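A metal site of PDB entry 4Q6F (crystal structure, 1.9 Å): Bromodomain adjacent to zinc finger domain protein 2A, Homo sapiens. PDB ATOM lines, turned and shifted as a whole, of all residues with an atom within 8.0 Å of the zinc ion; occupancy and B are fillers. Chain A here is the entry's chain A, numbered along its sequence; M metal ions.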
ATOM      1  N   THR A   8     -14.475 -18.392 -31.408  1.00  0.00           N
ATOM      2  CA  THR A   8     -13.018 -18.519 -31.330  1.00  0.00           C
ATOM      3  C   THR A   8     -12.372 -17.213 -31.786  1.00  0.00           C
ATOM      4  O   THR A   8     -12.997 -16.396 -32.454  1.00  0.00           O
ATOM      5  CB  THR A   8     -12.553 -19.701 -32.174  1.00  0.00           C
ATOM      6  OG1 THR A   8     -13.032 -19.512 -33.505  1.00  0.00           O
ATOM      7  CG2 THR A   8     -13.136 -21.002 -31.638  1.00  0.00           C
ATOM      8  N   CYS A   9     -11.120 -17.005 -31.390  1.00  0.00           N
ATOM      9  CA  CYS A   9     -10.395 -15.795 -31.719  1.00  0.00           C
ATOM     10  C   CYS A   9      -9.948 -15.818 -33.160  1.00  0.00           C
ATOM     11  O   CYS A   9      -9.382 -16.800 -33.623  1.00  0.00           O
ATOM     12  CB  CYS A   9      -9.195 -15.685 -30.797  1.00  0.00           C
ATOM     13  SG  CYS A   9      -8.050 -14.365 -31.174  1.00  0.00           S
ATOM     14  N   LEU A  10     -10.186 -14.721 -33.873  1.00  0.00           N
ATOM     15  CA  LEU A  10      -9.790 -14.610 -35.267  1.00  0.00           C
ATOM     16  C   LEU A  10      -8.298 -14.754 -35.467  1.00  0.00           C
ATOM     17  O   LEU A  10      -7.862 -15.190 -36.520  1.00  0.00           O
ATOM     18  CB  LEU A  10     -10.197 -13.244 -35.860  1.00  0.00           C
ATOM     19  CG  LEU A  10     -11.639 -13.100 -36.330  1.00  0.00           C
ATOM     20  CD1 LEU A  10     -11.968 -11.637 -36.592  1.00  0.00           C
ATOM     21  CD2 LEU A  10     -11.891 -13.957 -37.573  1.00  0.00           C
ATOM     22  N   VAL A  11      -7.494 -14.372 -34.481  1.00  0.00           N
ATOM     23  CA  VAL A  11      -6.052 -14.317 -34.637  1.00  0.00           C
ATOM     24  C   VAL A  11      -5.431 -15.683 -34.335  1.00  0.00           C
ATOM     25  O   VAL A  11      -4.716 -16.228 -35.182  1.00  0.00           O
ATOM     26  CB  VAL A  11      -5.433 -13.261 -33.683  1.00  0.00           C
ATOM     27  CG1 VAL A  11      -3.932 -13.157 -33.845  1.00  0.00           C
ATOM     28  CG2 VAL A  11      -6.079 -11.902 -33.948  1.00  0.00           C
ATOM     29  N   CYS A  12      -5.695 -16.209 -33.138  1.00  0.00           N
ATOM     30  CA  CYS A  12      -5.039 -17.419 -32.646  1.00  0.00           C
ATOM     31  C   CYS A  12      -5.904 -18.678 -32.858  1.00  0.00           C
ATOM     32  O   CYS A  12      -5.434 -19.764 -32.672  1.00  0.00           O
ATOM     33  CB  CYS A  12      -4.682 -17.298 -31.171  1.00  0.00           C
ATOM     34  SG  CYS A  12      -6.063 -17.426 -30.016  1.00  0.00           S
ATOM     35  N   ARG A  13      -7.173 -18.496 -33.207  1.00  0.00           N
ATOM     36  CA  ARG A  13      -8.119 -19.604 -33.477  1.00  0.00           C
ATOM     37  C   ARG A  13      -8.582 -20.436 -32.303  1.00  0.00           C
ATOM     38  O   ARG A  13      -9.332 -21.395 -32.515  1.00  0.00           O
ATOM     39  CB  ARG A  13      -7.619 -20.530 -34.598  1.00  0.00           C
ATOM     40  CG  ARG A  13      -6.989 -19.851 -35.777  1.00  0.00           C
ATOM     41  CD  ARG A  13      -7.858 -18.754 -36.370  1.00  0.00           C
ATOM     42  NE  ARG A  13      -7.012 -17.775 -37.073  1.00  0.00           N
ATOM     43  CZ  ARG A  13      -6.846 -17.697 -38.407  1.00  0.00           C
ATOM     44  NH1 ARG A  13      -7.466 -18.533 -39.229  1.00  0.00           N
ATOM     45  NH2 ARG A  13      -6.038 -16.762 -38.907  1.00  0.00           N
ATOM     46  N   LYS A  14      -8.169 -20.084 -31.076  1.00  0.00           N
ATOM     47  CA  LYS A  14      -8.645 -20.753 -29.858  1.00  0.00           C
ATOM     48  C   LYS A  14      -9.841 -20.072 -29.205  1.00  0.00           C
ATOM     49  O   LYS A  14     -10.101 -18.867 -29.418  1.00  0.00           O
ATOM     50  CB  LYS A  14      -7.532 -20.814 -28.838  1.00  0.00           C
ATOM     51  CG  LYS A  14      -6.307 -21.584 -29.312  1.00  0.00           C
ATOM     52  CD  LYS A  14      -5.243 -21.463 -28.247  1.00  0.00           C
ATOM     53  CE  LYS A  14      -3.909 -22.077 -28.650  1.00  0.00           C
ATOM     54  NZ  LYS A  14      -2.891 -21.615 -27.653  1.00  0.00           N
ATOM     55  N   GLY A  15     -10.574 -20.848 -28.419  1.00  0.00           N
ATOM     56  CA  GLY A  15     -11.772 -20.341 -27.744  1.00  0.00           C
ATOM     57  C   GLY A  15     -11.595 -20.218 -26.243  1.00  0.00           C
ATOM     58  O   GLY A  15     -12.588 -20.074 -25.523  1.00  0.00           O
ATOM     59  N   ASP A  16     -10.360 -20.260 -25.771  1.00  0.00           N
ATOM     60  CA  ASP A  16     -10.090 -20.256 -24.328  1.00  0.00           C
ATOM     61  C   ASP A  16     -10.029 -18.808 -23.793  1.00  0.00           C
ATOM     62  O   ASP A  16     -10.149 -17.844 -24.579  1.00  0.00           O
ATOM     63  CB  ASP A  16      -8.759 -20.951 -24.053  1.00  0.00           C
ATOM     64  CG  ASP A  16      -7.585 -20.310 -24.792  1.00  0.00           C
ATOM     65  OD1 ASP A  16      -7.777 -19.470 -25.717  1.00  0.00           O
ATOM     66  OD2 ASP A  16      -6.454 -20.643 -24.442  1.00  0.00           O
ATOM     67  N   ASN A  17      -9.863 -18.670 -22.469  1.00  0.00           N
ATOM     68  CA  ASN A  17      -9.730 -17.372 -21.826  1.00  0.00           C
ATOM     69  C   ASN A  17     -10.895 -16.462 -22.214  1.00  0.00           C
ATOM     70  O   ASN A  17     -10.720 -15.292 -22.689  1.00  0.00           O
ATOM     71  CB  ASN A  17      -8.382 -16.735 -22.158  1.00  0.00           C
ATOM     72  CG  ASN A  17      -7.199 -17.497 -21.594  1.00  0.00           C
ATOM     73  OD1 ASN A  17      -6.120 -17.514 -22.155  1.00  0.00           O
ATOM     74  ND2 ASN A  17      -7.389 -18.092 -20.462  1.00  0.00           N
ATOM     75  N   PHE A  20     -11.329 -12.673 -21.699  1.00  0.00           N
ATOM     76  CA  PHE A  20     -10.488 -11.817 -22.567  1.00  0.00           C
ATOM     77  C   PHE A  20     -10.968 -11.813 -24.003  1.00  0.00           C
ATOM     78  O   PHE A  20     -10.399 -11.106 -24.839  1.00  0.00           O
ATOM     79  CB  PHE A  20      -9.042 -12.342 -22.528  1.00  0.00           C
ATOM     80  CG  PHE A  20      -8.370 -12.151 -21.184  1.00  0.00           C
ATOM     81  CD1 PHE A  20      -8.450 -13.122 -20.199  1.00  0.00           C
ATOM     82  CD2 PHE A  20      -7.654 -10.985 -20.915  1.00  0.00           C
ATOM     83  CE1 PHE A  20      -7.815 -12.928 -18.973  1.00  0.00           C
ATOM     84  CE2 PHE A  20      -7.014 -10.802 -19.696  1.00  0.00           C
ATOM     85  CZ  PHE A  20      -7.104 -11.769 -18.725  1.00  0.00           C
ATOM     86  N   LEU A  21     -12.010 -12.608 -24.317  1.00  0.00           N
ATOM     87  CA  LEU A  21     -12.352 -12.922 -25.699  1.00  0.00           C
ATOM     88  C   LEU A  21     -13.500 -12.023 -26.115  1.00  0.00           C
ATOM     89  O   LEU A  21     -14.664 -12.252 -25.778  1.00  0.00           O
ATOM     90  CB  LEU A  21     -12.647 -14.411 -25.904  1.00  0.00           C
ATOM     91  CG  LEU A  21     -12.319 -14.978 -27.284  1.00  0.00           C
ATOM     92  CD1 LEU A  21     -12.596 -16.488 -27.326  1.00  0.00           C
ATOM     93  CD2 LEU A  21     -13.102 -14.295 -28.382  1.00  0.00           C
ATOM     94  N   GLY A  30     -14.835 -13.236 -32.988  1.00  0.00           N
ATOM     95  CA  GLY A  30     -14.203 -12.727 -31.769  1.00  0.00           C
ATOM     96  C   GLY A  30     -12.711 -12.519 -31.878  1.00  0.00           C
ATOM     97  O   GLY A  30     -12.065 -12.840 -32.894  1.00  0.00           O
ATOM     98  N   CYS A  31     -12.161 -11.916 -30.828  1.00  0.00           N
ATOM     99  CA  CYS A  31     -10.743 -11.711 -30.769  1.00  0.00           C
ATOM    100  C   CYS A  31     -10.337 -11.515 -29.337  1.00  0.00           C
ATOM    101  O   CYS A  31     -10.926 -10.680 -28.639  1.00  0.00           O
ATOM    102  CB  CYS A  31     -10.391 -10.479 -31.592  1.00  0.00           C
ATOM    103  SG  CYS A  31      -8.641 -10.164 -31.774  1.00  0.00           S
ATOM    104  N   HIS A  32      -9.339 -12.275 -28.881  1.00  0.00           N
ATOM    105  CA  HIS A  32      -8.743 -11.989 -27.572  1.00  0.00           C
ATOM    106  C   HIS A  32      -8.198 -10.592 -27.557  1.00  0.00           C
ATOM    107  O   HIS A  32      -7.491 -10.192 -28.487  1.00  0.00           O
ATOM    108  CB  HIS A  32      -7.606 -12.950 -27.194  1.00  0.00           C
ATOM    109  CG  HIS A  32      -8.050 -14.363 -27.038  1.00  0.00           C
ATOM    110  ND1 HIS A  32      -7.656 -15.358 -27.907  1.00  0.00           N
ATOM    111  CD2 HIS A  32      -8.856 -14.946 -26.128  1.00  0.00           C
ATOM    112  CE1 HIS A  32      -8.208 -16.503 -27.529  1.00  0.00           C
ATOM    113  NE2 HIS A  32      -8.946 -16.273 -26.461  1.00  0.00           N
ATOM    114  N   ILE A  33      -8.454  -9.864 -26.486  1.00  0.00           N
ATOM    115  CA  ILE A  33      -7.792  -8.553 -26.376  1.00  0.00           C
ATOM    116  C   ILE A  33      -6.249  -8.611 -26.463  1.00  0.00           C
ATOM    117  O   ILE A  33      -5.598  -7.691 -26.994  1.00  0.00           O
ATOM    118  CB  ILE A  33      -8.246  -7.740 -25.154  1.00  0.00           C
ATOM    119  CG1 ILE A  33      -7.766  -8.372 -23.839  1.00  0.00           C
ATOM    120  CG2 ILE A  33      -9.769  -7.532 -25.153  1.00  0.00           C
ATOM    121  CD1 ILE A  33      -7.914  -7.429 -22.665  1.00  0.00           C
ATOM    122  N   TYR A  34      -5.669  -9.708 -25.978  1.00  0.00           N
ATOM    123  CA  TYR A  34      -4.214  -9.850 -26.006  1.00  0.00           C
ATOM    124  C   TYR A  34      -3.652 -10.281 -27.351  1.00  0.00           C
ATOM    125  O   TYR A  34      -2.418 -10.166 -27.539  1.00  0.00           O
ATOM    126  CB  TYR A  34      -3.700 -10.801 -24.927  1.00  0.00           C
ATOM    127  CG  TYR A  34      -4.369 -12.159 -24.879  1.00  0.00           C
ATOM    128  CD1 TYR A  34      -4.082 -13.158 -25.819  1.00  0.00           C
ATOM    129  CD2 TYR A  34      -5.268 -12.481 -23.840  1.00  0.00           C
ATOM    130  CE1 TYR A  34      -4.658 -14.410 -25.732  1.00  0.00           C
ATOM    131  CE2 TYR A  34      -5.843 -13.751 -23.766  1.00  0.00           C
ATOM    132  CZ  TYR A  34      -5.517 -14.698 -24.704  1.00  0.00           C
ATOM    133  OH  TYR A  34      -6.077 -15.961 -24.646  1.00  0.00           O
ATOM    134  N   CYS A  35      -4.502 -10.736 -28.253  1.00  0.00           N
ATOM    135  CA  CYS A  35      -4.070 -11.045 -29.645  1.00  0.00           C
ATOM    136  C   CYS A  35      -4.192  -9.819 -30.584  1.00  0.00           C
ATOM    137  O   CYS A  35      -3.589  -9.770 -31.684  1.00  0.00           O
ATOM    138  CB  CYS A  35      -4.917 -12.220 -30.195  1.00  0.00           C
ATOM    139  SG  CYS A  35      -4.624 -13.819 -29.350  1.00  0.00           S
ATOM    140  N   HIS A  36      -4.990  -8.863 -30.162  1.00  0.00           N
ATOM    141  CA  HIS A  36      -5.304  -7.709 -30.979  1.00  0.00           C
ATOM    142  C   HIS A  36      -4.066  -6.870 -31.128  1.00  0.00           C
ATOM    143  O   HIS A  36      -3.285  -6.696 -30.180  1.00  0.00           O
ATOM    144  CB  HIS A  36      -6.426  -6.890 -30.322  1.00  0.00           C
ATOM    145  CG  HIS A  36      -7.028  -5.863 -31.228  1.00  0.00           C
ATOM    146  ND1 HIS A  36      -6.448  -4.633 -31.463  1.00  0.00           N
ATOM    147  CD2 HIS A  36      -8.195  -5.867 -31.909  1.00  0.00           C
ATOM    148  CE1 HIS A  36      -7.199  -3.955 -32.301  1.00  0.00           C
ATOM    149  NE2 HIS A  36      -8.252  -4.688 -32.609  1.00  0.00           N
HETATM  150 ZN    ZN M   1      -6.447 -15.125 -29.602  1.00  0.00          ZN
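OH of Tyr 34 sits close to NE2 of His 32.
NE2 of His 32 sits at hydrogen-bond distance from O of Asp 16 (2.7 Å).
SG of Cys 12 lies close to N of Lys 14, 3.6 Å away.
SG of Cys 9 lies close to N of Val 11, 3.4 Å away.
The backbone carbonyl oxygen of Lys 14 lies within hydrogen-bond range of the backbone NH of Cys 9 (2.9 Å).
Of the 19 residues printed, 4 come within 4 Å of the zinc ion.
The zinc ion is bound by a ring nitrogen (ND1) of His 32 (2.1 Å), the side-chain sulfur of Cys 35 (2.3 Å), the side-chain sulfur of Cys 12 (2.4 Å) and the side-chain sulfur of Cys 9 (2.4 Å).
The zinc ion has four donor atoms within binding distance.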
